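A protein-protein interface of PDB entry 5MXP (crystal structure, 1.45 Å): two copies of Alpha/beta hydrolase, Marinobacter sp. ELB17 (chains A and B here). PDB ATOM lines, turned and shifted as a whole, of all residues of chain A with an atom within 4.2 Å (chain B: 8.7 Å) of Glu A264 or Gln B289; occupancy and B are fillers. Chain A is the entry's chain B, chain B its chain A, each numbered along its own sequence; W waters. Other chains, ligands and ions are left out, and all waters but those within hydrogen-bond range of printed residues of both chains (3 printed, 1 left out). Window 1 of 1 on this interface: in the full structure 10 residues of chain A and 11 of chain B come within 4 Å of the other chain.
The side-chain amide nitrogen (NE2) of Gln B289 lies close to the guanidinium group (NH1) of Arg A257. The backbone carbonyl oxygen (O) of Cys B294 lies within hydrogen-bond range of the side-chain amide nitrogen (ND2) of Asn A262, at 3.4 Å. OE1 of Gln B289 lies within hydrogen-bond range of N of Thr A265. The side-chain carboxylate (OE1) of Glu B264 lies within salt-bridge range of the guanidinium group (NH2) of Arg A293, at 3.1 Å.
Arg A293 touches Glu B264, but with the chains exchanged Glu A264 does not touch Arg B293 (7.0 Å). Arg A293 touches Trp B290, but with the chains exchanged Trp A290 does not touch Arg B293 (7.6 Å). Arg A293 touches its own counterpart, Arg B293. Of the 11 pairs that touch across the chains among the printed residues, 1 has its exchanged pair printed and touching as well.
Among the printed residues, merely in contact across the chains: Arg A257 with Gln B285, Glu A264 with Gln B289, Arg A293 with Gln B289, Arg A293 with Trp B290, Arg A293 with Arg B293, Arg A293 with Cys B294 and Arg A293 with Leu B296.
Glu A264 touches one residue of chain B. Of chain A, only Arg A257 (3.2 Å), Glu A264 (3.2 Å), Thr A265 (2.9 Å) and Arg A293 (3.7 Å) come within 4 Å of Gln B289. No residue of chain B comes within 4 Å of Leu A263. Of the printed residues of chain B, Arg A257 touches Gln B285 (3.4 Å) and Gln B289 (3.2 Å). Printed residues of chain A within 4 Å of Cys B294: Asn A262 (3.4 Å) and Arg A293 (3.8 Å). Printed residues of chain B within 4 Å of Arg A293: Glu B264, Gln B289, Trp B290, Arg B293, Cys B294 and Leu B296. The nearest printed residue of chain A that does not touch Cys B294 is Trp A290 (4.7 Å).
Of the 10 printed residues of chain A, 5 touch a printed residue of chain B. Printed residues of chain A that touch a printed residue of chain B: Arg A257, Asn A262, Glu A264, Thr A265 and Arg A293. Hydrophobic or aromatic side chains of chain B within 4 Å of the printed part of chain A: Trp B290 and Leu B296. Along chain B the printed residues that touch a printed residue of chain A span positions 264 to 296. Among the printed residues, 11 pairs touch across the chains.
Water W3 lies within hydrogen-bond range of OE2 of Glu B264 (2.5 Å) and N of Arg A293 (3.4 Å). Water W1 bridges the side-chain amide oxygen of Gln B289 (2.7 Å) and the backbone carbonyl oxygen of Thr A265 (3.1 Å). Water W2 lies within hydrogen-bond range of the backbone carbonyl oxygen of Ala B286 (2.8 Å) and the guanidinium group of Arg A293 (3.1 Å).
N of Leu A239 sits at hydrogen-bond distance from O of Glu A264 (2.8 Å). O of Asn A262 sits at hydrogen-bond distance from N of Lys A237. OG1 of Thr A265 sits at hydrogen-bond distance from NH1 of Arg A257 (2.7 Å). O of Lys A237 lies within hydrogen-bond range of N of Glu A264. The side-chain carboxylate of Glu B53 sits at hydrogen-bond distance from the side-chain amide nitrogen of Gln B285, 2.5 Å away. The side-chain carboxylate (OE1) of Glu A264 is in salt-bridge range of the guanidinium group (NH1) of Arg A293.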
ATOM      1  N   LYS A 237       8.041   9.547 -14.354  1.00  0.00           N
ATOM      2  CA  LYS A 237       8.017   8.153 -14.088  1.00  0.00           C
ATOM      3  C   LYS A 237       8.249   7.385 -15.393  1.00  0.00           C
ATOM      4  O   LYS A 237       7.828   7.847 -16.445  1.00  0.00           O
ATOM      5  CB  LYS A 237       6.633   7.829 -13.587  1.00  0.00           C
ATOM      6  CG  LYS A 237       6.281   8.400 -12.228  1.00  0.00           C
ATOM      7  CD  LYS A 237       4.797   8.214 -11.873  1.00  0.00           C
ATOM      8  CE  LYS A 237       4.315   9.323 -10.910  1.00  0.00           C
ATOM      9  NZ  LYS A 237       4.181  10.659 -11.543  1.00  0.00           N
ATOM     10  N   LEU A 238       8.909   6.232 -15.264  1.00  0.00           N
ATOM     11  CA  LEU A 238       9.175   5.407 -16.418  1.00  0.00           C
ATOM     12  C   LEU A 238       8.832   4.004 -15.929  1.00  0.00           C
ATOM     13  O   LEU A 238       9.458   3.510 -14.991  1.00  0.00           O
ATOM     14  CB  LEU A 238      10.639   5.409 -16.835  1.00  0.00           C
ATOM     15  CG  LEU A 238      11.061   4.434 -17.944  1.00  0.00           C
ATOM     16  CD1 LEU A 238      10.368   4.707 -19.280  1.00  0.00           C
ATOM     17  CD2 LEU A 238      12.557   4.526 -18.104  1.00  0.00           C
ATOM     18  N   LEU A 239       7.902   3.352 -16.641  1.00  0.00           N
ATOM     19  CA  LEU A 239       7.570   1.930 -16.414  1.00  0.00           C
ATOM     20  C   LEU A 239       8.115   1.122 -17.590  1.00  0.00           C
ATOM     21  O   LEU A 239       7.690   1.305 -18.704  1.00  0.00           O
ATOM     22  CB  LEU A 239       6.079   1.776 -16.345  1.00  0.00           C
ATOM     23  CG  LEU A 239       5.489   0.393 -16.297  1.00  0.00           C
ATOM     24  CD1 LEU A 239       6.060  -0.411 -15.154  1.00  0.00           C
ATOM     25  CD2 LEU A 239       3.980   0.521 -16.205  1.00  0.00           C
ATOM     26  N   ARG A 257      -0.461   3.675 -17.517  1.00  0.00           N
ATOM     27  CA  ARG A 257      -0.315   4.727 -18.515  1.00  0.00           C
ATOM     28  C   ARG A 257      -1.277   5.875 -18.179  1.00  0.00           C
ATOM     29  O   ARG A 257      -0.934   7.079 -18.270  1.00  0.00           O
ATOM     30  CB  ARG A 257      -0.664   4.234 -19.952  1.00  0.00           C
ATOM     31  CG  ARG A 257       0.319   3.365 -20.751  1.00  0.00           C
ATOM     32  CD  ARG A 257      -0.292   2.790 -22.062  1.00  0.00           C
ATOM     33  NE  ARG A 257       0.507   1.678 -22.548  1.00  0.00           N
ATOM     34  CZ  ARG A 257       1.724   1.827 -23.059  1.00  0.00           C
ATOM     35  NH1 ARG A 257       2.226   3.034 -23.269  1.00  0.00           N
ATOM     36  NH2 ARG A 257       2.421   0.756 -23.435  1.00  0.00           N
ATOM     37  N   ASN A 262       2.486  11.744 -15.921  1.00  0.00           N
ATOM     38  CA  ASN A 262       3.845  11.879 -16.462  1.00  0.00           C
ATOM     39  C   ASN A 262       4.558  10.532 -16.540  1.00  0.00           C
ATOM     40  O   ASN A 262       5.731  10.459 -16.240  1.00  0.00           O
ATOM     41  CB  ASN A 262       4.649  12.872 -15.571  1.00  0.00           C
ATOM     42  CG  ASN A 262       5.870  13.417 -16.303  1.00  0.00           C
ATOM     43  OD1 ASN A 262       6.009  13.138 -17.543  1.00  0.00           O
ATOM     44  ND2 ASN A 262       6.730  14.241 -15.589  1.00  0.00           N
ATOM     45  N   LEU A 263       3.828   9.525 -16.960  1.00  0.00           N
ATOM     46  CA  LEU A 263       4.376   8.192 -17.066  1.00  0.00           C
ATOM     47  C   LEU A 263       4.759   7.879 -18.471  1.00  0.00           C
ATOM     48  O   LEU A 263       3.935   7.911 -19.365  1.00  0.00           O
ATOM     49  CB  LEU A 263       3.369   7.146 -16.567  1.00  0.00           C
ATOM     50  CG  LEU A 263       4.009   5.758 -16.666  1.00  0.00           C
ATOM     51  CD1 LEU A 263       4.759   5.461 -15.435  1.00  0.00           C
ATOM     52  CD2 LEU A 263       2.983   4.703 -16.957  1.00  0.00           C
ATOM     53  N   GLU A 264       6.025   7.526 -18.676  1.00  0.00           N
ATOM     54  CA  GLU A 264       6.513   7.020 -19.984  1.00  0.00           C
ATOM     55  C   GLU A 264       6.565   5.512 -19.788  1.00  0.00           C
ATOM     56  O   GLU A 264       6.772   4.983 -18.664  1.00  0.00           O
ATOM     57  CB  GLU A 264       7.899   7.552 -20.270  1.00  0.00           C
ATOM     58  CG  GLU A 264       8.609   6.928 -21.495  1.00  0.00           C
ATOM     59  CD  GLU A 264       9.837   7.664 -21.972  1.00  0.00           C
ATOM     60  OE1 GLU A 264       9.951   8.820 -21.671  1.00  0.00           O
ATOM     61  OE2 GLU A 264      10.682   7.065 -22.691  1.00  0.00           O
ATOM     62  N   THR A 265       6.396   4.802 -20.911  1.00  0.00           N
ATOM     63  CA  THR A 265       6.566   3.396 -20.911  1.00  0.00           C
ATOM     64  C   THR A 265       7.659   2.987 -21.857  1.00  0.00           C
ATOM     65  O   THR A 265       7.907   3.648 -22.888  1.00  0.00           O
ATOM     66  CB  THR A 265       5.276   2.661 -21.262  1.00  0.00           C
ATOM     67  OG1 THR A 265       4.810   3.148 -22.519  1.00  0.00           O
ATOM     68  CG2 THR A 265       4.228   2.905 -20.226  1.00  0.00           C
ATOM     69  N   TRP A 290      14.924   8.314 -21.403  1.00  0.00           N
ATOM     70  CA  TRP A 290      13.928   8.955 -20.611  1.00  0.00           C
ATOM     71  C   TRP A 290      14.571  10.061 -19.734  1.00  0.00           C
ATOM     72  O   TRP A 290      14.005  11.195 -19.641  1.00  0.00           O
ATOM     73  CB  TRP A 290      13.278   7.913 -19.716  1.00  0.00           C
ATOM     74  CG  TRP A 290      12.418   8.383 -18.519  1.00  0.00           C
ATOM     75  CD1 TRP A 290      11.184   8.945 -18.548  1.00  0.00           C
ATOM     76  CD2 TRP A 290      12.800   8.309 -17.159  1.00  0.00           C
ATOM     77  NE1 TRP A 290      10.763   9.213 -17.259  1.00  0.00           N
ATOM     78  CE2 TRP A 290      11.737   8.832 -16.382  1.00  0.00           C
ATOM     79  CE3 TRP A 290      13.978   7.889 -16.507  1.00  0.00           C
ATOM     80  CZ2 TRP A 290      11.802   8.931 -14.972  1.00  0.00           C
ATOM     81  CZ3 TRP A 290      14.020   7.947 -15.087  1.00  0.00           C
ATOM     82  CH2 TRP A 290      12.908   8.487 -14.321  1.00  0.00           C
ATOM     83  N   ARG A 293      15.181  12.946 -22.021  1.00  0.00           N
ATOM     84  CA  ARG A 293      13.912  13.601 -22.352  1.00  0.00           C
ATOM     85  C   ARG A 293      13.411  14.480 -21.245  1.00  0.00           C
ATOM     86  O   ARG A 293      12.775  15.504 -21.492  1.00  0.00           O
ATOM     87  CB  ARG A 293      12.846  12.528 -22.653  1.00  0.00           C
ATOM     88  CG  ARG A 293      11.601  13.055 -23.351  1.00  0.00           C
ATOM     89  CD  ARG A 293      10.667  11.886 -23.679  1.00  0.00           C
ATOM     90  NE  ARG A 293      10.904  11.387 -25.062  1.00  0.00           N
ATOM     91  CZ  ARG A 293      10.255  10.336 -25.553  1.00  0.00           C
ATOM     92  NH1 ARG A 293       9.286   9.767 -24.845  1.00  0.00           N
ATOM     93  NH2 ARG A 293      10.498   9.873 -26.782  1.00  0.00           N
ATOM     94  N   GLU B  53      -5.070   7.343 -29.491  1.00  0.00           N
ATOM     95  CA  GLU B  53      -4.013   7.607 -28.513  1.00  0.00           C
ATOM     96  C   GLU B  53      -3.523   9.013 -28.588  1.00  0.00           C
ATOM     97  O   GLU B  53      -2.878   9.493 -27.660  1.00  0.00           O
ATOM     98  CB  GLU B  53      -2.833   6.654 -28.660  1.00  0.00           C
ATOM     99  CG  GLU B  53      -3.241   5.192 -28.719  1.00  0.00           C
ATOM    100  CD  GLU B  53      -3.959   4.718 -27.467  1.00  0.00           C
ATOM    101  OE1 GLU B  53      -3.667   5.224 -26.342  1.00  0.00           O
ATOM    102  OE2 GLU B  53      -4.870   3.889 -27.570  1.00  0.00           O
ATOM    103  N   LEU B  54      -3.833   9.691 -29.709  1.00  0.00           N
ATOM    104  CA  LEU B  54      -3.320  11.060 -29.945  1.00  0.00           C
ATOM    105  C   LEU B  54      -4.402  12.123 -29.928  1.00  0.00           C
ATOM    106  O   LEU B  54      -4.108  13.316 -30.079  1.00  0.00           O
ATOM    107  CB  LEU B  54      -2.582  11.104 -31.291  1.00  0.00           C
ATOM    108  CG  LEU B  54      -1.291  10.254 -31.263  1.00  0.00           C
ATOM    109  CD1 LEU B  54      -0.759   9.854 -32.545  1.00  0.00           C
ATOM    110  CD2 LEU B  54      -0.220  10.944 -30.445  1.00  0.00           C
ATOM    111  N   LYS B  57      -3.976  15.831 -28.626  1.00  0.00           N
ATOM    112  CA  LYS B  57      -2.555  16.254 -28.716  1.00  0.00           C
ATOM    113  C   LYS B  57      -2.279  17.247 -29.828  1.00  0.00           C
ATOM    114  O   LYS B  57      -1.131  17.660 -30.003  1.00  0.00           O
ATOM    115  CB  LYS B  57      -1.590  15.064 -28.885  1.00  0.00           C
ATOM    116  CG  LYS B  57      -1.561  14.081 -27.725  1.00  0.00           C
ATOM    117  CD  LYS B  57      -0.896  14.695 -26.495  1.00  0.00           C
ATOM    118  CE  LYS B  57      -0.696  13.574 -25.495  1.00  0.00           C
ATOM    119  NZ  LYS B  57      -1.035  13.970 -24.116  1.00  0.00           N
ATOM    120  N   LEU B 238      11.381  10.574 -34.168  1.00  0.00           N
ATOM    121  CA  LEU B 238      11.034   9.410 -33.404  1.00  0.00           C
ATOM    122  C   LEU B 238      10.972   8.273 -34.348  1.00  0.00           C
ATOM    123  O   LEU B 238      10.178   8.335 -35.322  1.00  0.00           O
ATOM    124  CB  LEU B 238       9.680   9.606 -32.700  1.00  0.00           C
ATOM    125  CG  LEU B 238       9.102   8.377 -31.956  1.00  0.00           C
ATOM    126  CD1 LEU B 238       9.961   8.022 -30.743  1.00  0.00           C
ATOM    127  CD2 LEU B 238       7.649   8.661 -31.600  1.00  0.00           C
ATOM    128  N   GLU B 264      15.006   9.740 -31.199  1.00  0.00           N
ATOM    129  CA  GLU B 264      14.576   8.881 -30.085  1.00  0.00           C
ATOM    130  C   GLU B 264      13.895   7.681 -30.731  1.00  0.00           C
ATOM    131  O   GLU B 264      13.442   7.727 -31.844  1.00  0.00           O
ATOM    132  CB  GLU B 264      13.594   9.656 -29.196  1.00  0.00           C
ATOM    133  CG  GLU B 264      14.400  10.711 -28.396  1.00  0.00           C
ATOM    134  CD  GLU B 264      13.534  11.601 -27.507  1.00  0.00           C
ATOM    135  OE1 GLU B 264      12.502  11.976 -27.992  1.00  0.00           O
ATOM    136  OE2 GLU B 264      13.899  11.987 -26.381  1.00  0.00           O
ATOM    137  N   THR B 265      13.813   6.636 -29.950  1.00  0.00           N
ATOM    138  CA  THR B 265      13.253   5.373 -30.465  1.00  0.00           C
ATOM    139  C   THR B 265      12.221   4.842 -29.510  1.00  0.00           C
ATOM    140  O   THR B 265      12.254   5.100 -28.284  1.00  0.00           O
ATOM    141  CB  THR B 265      14.333   4.286 -30.643  1.00  0.00           C
ATOM    142  OG1 THR B 265      15.065   4.100 -29.433  1.00  0.00           O
ATOM    143  CG2 THR B 265      15.258   4.631 -31.769  1.00  0.00           C
ATOM    144  N   ALA B 266      11.364   3.985 -30.028  1.00  0.00           N
ATOM    145  CA  ALA B 266      10.386   3.277 -29.220  1.00  0.00           C
ATOM    146  C   ALA B 266      10.153   1.914 -29.848  1.00  0.00           C
ATOM    147  O   ALA B 266       9.721   1.798 -31.012  1.00  0.00           O
ATOM    148  CB  ALA B 266       9.090   4.043 -29.191  1.00  0.00           C
ATOM    149  N   GLN B 281      -1.878   0.582 -30.227  1.00  0.00           N
ATOM    150  CA  GLN B 281      -1.926   1.347 -28.980  1.00  0.00           C
ATOM    151  C   GLN B 281      -0.536   1.759 -28.588  1.00  0.00           C
ATOM    152  O   GLN B 281      -0.291   2.958 -28.221  1.00  0.00           O
ATOM    153  CB  GLN B 281      -2.621   0.581 -27.867  1.00  0.00           C
ATOM    154  CG  GLN B 281      -4.132   0.388 -28.111  1.00  0.00           C
ATOM    155  CD  GLN B 281      -4.524  -0.724 -29.055  1.00  0.00           C
ATOM    156  OE1 GLN B 281      -3.782  -1.721 -29.237  1.00  0.00           O
ATOM    157  NE2 GLN B 281      -5.695  -0.559 -29.680  1.00  0.00           N
ATOM    158  N   LYS B 282       0.399   0.828 -28.609  1.00  0.00           N
ATOM    159  CA  LYS B 282       1.791   1.136 -28.293  1.00  0.00           C
ATOM    160  C   LYS B 282       2.365   2.173 -29.229  1.00  0.00           C
ATOM    161  O   LYS B 282       3.143   3.029 -28.820  1.00  0.00           O
ATOM    162  CB  LYS B 282       2.660  -0.111 -28.307  1.00  0.00           C
ATOM    163  CG  LYS B 282       2.421  -1.058 -27.145  1.00  0.00           C
ATOM    164  CD  LYS B 282       3.511  -2.128 -27.117  1.00  0.00           C
ATOM    165  CE  LYS B 282       3.319  -3.077 -25.972  1.00  0.00           C
ATOM    166  NZ  LYS B 282       2.359  -4.149 -26.368  1.00  0.00           N
ATOM    167  N   ILE B 283       2.025   2.085 -30.506  1.00  0.00           N
ATOM    168  CA  ILE B 283       2.532   3.081 -31.463  1.00  0.00           C
ATOM    169  C   ILE B 283       1.990   4.462 -31.141  1.00  0.00           C
ATOM    170  O   ILE B 283       2.758   5.475 -31.061  1.00  0.00           O
ATOM    171  CB  ILE B 283       2.149   2.682 -32.925  1.00  0.00           C
ATOM    172  CG1 ILE B 283       2.963   1.481 -33.322  1.00  0.00           C
ATOM    173  CG2 ILE B 283       2.328   3.837 -33.905  1.00  0.00           C
ATOM    174  CD1 ILE B 283       2.418   0.764 -34.501  1.00  0.00           C
ATOM    175  N   GLY B 284       0.678   4.543 -30.941  1.00  0.00           N
ATOM    176  CA  GLY B 284       0.086   5.801 -30.579  1.00  0.00           C
ATOM    177  C   GLY B 284       0.660   6.371 -29.315  1.00  0.00           C
ATOM    178  O   GLY B 284       0.940   7.557 -29.227  1.00  0.00           O
ATOM    179  N   GLN B 285       0.820   5.533 -28.310  1.00  0.00           N
ATOM    180  CA  GLN B 285       1.344   6.002 -27.011  1.00  0.00           C
ATOM    181  C   GLN B 285       2.769   6.409 -27.156  1.00  0.00           C
ATOM    182  O   GLN B 285       3.195   7.365 -26.548  1.00  0.00           O
ATOM    183  CB  GLN B 285       1.181   4.906 -25.968  1.00  0.00           C
ATOM    184  CG  GLN B 285      -0.242   4.833 -25.413  1.00  0.00           C
ATOM    185  CD  GLN B 285      -0.708   6.164 -24.788  1.00  0.00           C
ATOM    186  OE1 GLN B 285       0.082   6.898 -24.158  1.00  0.00           O
ATOM    187  NE2 GLN B 285      -1.970   6.543 -25.090  1.00  0.00           N
ATOM    188  N   ALA B 286       3.553   5.754 -27.978  1.00  0.00           N
ATOM    189  CA  ALA B 286       4.935   6.204 -28.223  1.00  0.00           C
ATOM    190  C   ALA B 286       4.995   7.603 -28.784  1.00  0.00           C
ATOM    191  O   ALA B 286       5.809   8.429 -28.323  1.00  0.00           O
ATOM    192  CB  ALA B 286       5.706   5.225 -29.090  1.00  0.00           C
ATOM    193  N   ILE B 287       4.116   7.899 -29.741  1.00  0.00           N
ATOM    194  CA  ILE B 287       4.084   9.201 -30.344  1.00  0.00           C
ATOM    195  C   ILE B 287       3.611  10.157 -29.276  1.00  0.00           C
ATOM    196  O   ILE B 287       4.205  11.286 -29.133  1.00  0.00           O
ATOM    197  CB  ILE B 287       3.159   9.232 -31.580  1.00  0.00           C
ATOM    198  CG1 ILE B 287       3.672   8.272 -32.652  1.00  0.00           C
ATOM    199  CG2 ILE B 287       3.038  10.697 -32.091  1.00  0.00           C
ATOM    200  CD1 ILE B 287       2.645   7.881 -33.719  1.00  0.00           C
ATOM    201  N   ALA B 288       2.567   9.824 -28.538  1.00  0.00           N
ATOM    202  CA  ALA B 288       2.064  10.725 -27.504  1.00  0.00           C
ATOM    203  C   ALA B 288       3.123  11.085 -26.474  1.00  0.00           C
ATOM    204  O   ALA B 288       3.251  12.246 -26.123  1.00  0.00           O
ATOM    205  CB  ALA B 288       0.854  10.135 -26.818  1.00  0.00           C
ATOM    206  N   GLN B 289       3.879  10.104 -25.972  1.00  0.00           N
ATOM    207  CA  GLN B 289       4.878  10.335 -24.971  1.00  0.00           C
ATOM    208  C   GLN B 289       5.977  11.223 -25.519  1.00  0.00           C
ATOM    209  O   GLN B 289       6.426  12.144 -24.836  1.00  0.00           O
ATOM    210  CB  GLN B 289       5.445   9.016 -24.400  1.00  0.00           C
ATOM    211  CG  GLN B 289       4.332   8.267 -23.619  1.00  0.00           C
ATOM    212  CD  GLN B 289       4.714   6.794 -23.312  1.00  0.00           C
ATOM    213  OE1 GLN B 289       5.906   6.539 -23.230  1.00  0.00           O
ATOM    214  NE2 GLN B 289       3.736   5.843 -23.201  1.00  0.00           N
ATOM    215  N   TRP B 290       6.375  11.034 -26.767  1.00  0.00           N
ATOM    216  CA  TRP B 290       7.405  11.794 -27.396  1.00  0.00           C
ATOM    217  C   TRP B 290       6.938  13.246 -27.583  1.00  0.00           C
ATOM    218  O   TRP B 290       7.707  14.226 -27.336  1.00  0.00           O
ATOM    219  CB  TRP B 290       7.680  11.182 -28.752  1.00  0.00           C
ATOM    220  CG  TRP B 290       8.546  11.976 -29.768  1.00  0.00           C
ATOM    221  CD1 TRP B 290       9.895  12.234 -29.714  1.00  0.00           C
ATOM    222  CD2 TRP B 290       8.079  12.502 -30.962  1.00  0.00           C
ATOM    223  NE1 TRP B 290      10.321  12.883 -30.884  1.00  0.00           N
ATOM    224  CE2 TRP B 290       9.221  13.072 -31.672  1.00  0.00           C
ATOM    225  CE3 TRP B 290       6.823  12.593 -31.539  1.00  0.00           C
ATOM    226  CZ2 TRP B 290       9.106  13.668 -32.915  1.00  0.00           C
ATOM    227  CZ3 TRP B 290       6.710  13.171 -32.849  1.00  0.00           C
ATOM    228  CH2 TRP B 290       7.856  13.681 -33.507  1.00  0.00           C
ATOM    229  N   MET B 291       5.671  13.437 -28.002  1.00  0.00           N
ATOM    230  CA  MET B 291       5.153  14.847 -28.138  1.00  0.00           C
ATOM    231  C   MET B 291       5.100  15.545 -26.782  1.00  0.00           C
ATOM    232  O   MET B 291       5.487  16.770 -26.642  1.00  0.00           O
ATOM    233  CB  MET B 291       3.809  14.892 -28.773  1.00  0.00           C
ATOM    234  CG  MET B 291       3.830  14.435 -30.228  1.00  0.00           C
ATOM    235  SD  MET B 291       2.179  14.416 -30.919  1.00  0.00           S
ATOM    236  CE  MET B 291       1.995  16.199 -31.213  1.00  0.00           C
ATOM    237  N   ASP B 292       4.718  14.833 -25.735  1.00  0.00           N
ATOM    238  CA  ASP B 292       4.650  15.375 -24.348  1.00  0.00           C
ATOM    239  C   ASP B 292       5.937  15.695 -23.766  1.00  0.00           C
ATOM    240  O   ASP B 292       5.900  16.486 -22.829  1.00  0.00           O
ATOM    241  CB  ASP B 292       3.978  14.436 -23.401  1.00  0.00           C
ATOM    242  CG  ASP B 292       2.515  14.409 -23.556  1.00  0.00           C
ATOM    243  OD1 ASP B 292       1.997  15.333 -24.257  1.00  0.00           O
ATOM    244  OD2 ASP B 292       1.906  13.421 -23.014  1.00  0.00           O
ATOM    245  N   ARG B 293       7.075  15.158 -24.232  1.00  0.00           N
ATOM    246  CA  ARG B 293       8.401  15.604 -23.713  1.00  0.00           C
ATOM    247  C   ARG B 293       8.522  15.702 -22.216  1.00  0.00           C
ATOM    248  O   ARG B 293       9.047  16.670 -21.691  1.00  0.00           O
ATOM    249  CB  ARG B 293       8.869  16.961 -24.327  1.00  0.00           C
ATOM    250  CG  ARG B 293      10.395  17.073 -24.307  1.00  0.00           C
ATOM    251  CD  ARG B 293      10.921  18.130 -25.302  1.00  0.00           C
ATOM    252  NE  ARG B 293      10.964  19.474 -24.693  1.00  0.00           N
ATOM    253  CZ  ARG B 293      12.003  20.019 -24.053  1.00  0.00           C
ATOM    254  NH1 ARG B 293      11.872  21.248 -23.565  1.00  0.00           N
ATOM    255  NH2 ARG B 293      13.163  19.376 -23.888  1.00  0.00           N
ATOM    256  N   CYS B 294       7.989  14.685 -21.533  1.00  0.00           N
ATOM    257  CA  CYS B 294       8.136  14.521 -20.133  1.00  0.00           C
ATOM    258  C   CYS B 294       7.496  15.669 -19.359  1.00  0.00           C
ATOM    259  O   CYS B 294       7.893  15.957 -18.224  1.00  0.00           O
ATOM    260  CB  CYS B 294       9.611  14.261 -19.784  1.00  0.00           C
ATOM    261  SG  CYS B 294       9.835  13.749 -18.045  1.00  0.00           S
ATOM    262  N   GLY B 295       6.525  16.353 -19.990  1.00  0.00           N
ATOM    263  CA  GLY B 295       5.921  17.532 -19.256  1.00  0.00           C
ATOM    264  C   GLY B 295       6.770  18.792 -19.300  1.00  0.00           C
ATOM    265  O   GLY B 295       6.401  19.771 -18.656  1.00  0.00           O
ATOM    266  N   LEU B 296       7.900  18.781 -20.008  1.00  0.00           N
ATOM    267  CA  LEU B 296       8.685  20.000 -20.244  1.00  0.00           C
ATOM    268  C   LEU B 296       8.017  20.820 -21.374  1.00  0.00           C
ATOM    269  O   LEU B 296       8.167  22.069 -21.396  1.00  0.00           O
ATOM    270  CB  LEU B 296      10.128  19.652 -20.625  1.00  0.00           C
ATOM    271  CG  LEU B 296      10.960  18.767 -19.687  1.00  0.00           C
ATOM    272  CD1 LEU B 296      12.384  18.615 -20.239  1.00  0.00           C
ATOM    273  CD2 LEU B 296      10.992  19.252 -18.272  1.00  0.00           C
HETATM  274  O   HOH W   1       7.116   5.356 -25.376  1.00  0.00           O
HETATM  275  O   HOH W   2       8.286   7.706 -27.324  1.00  0.00           O
HETATM  276  O   HOH W   3      15.904  11.425 -24.974  1.00  0.00           O
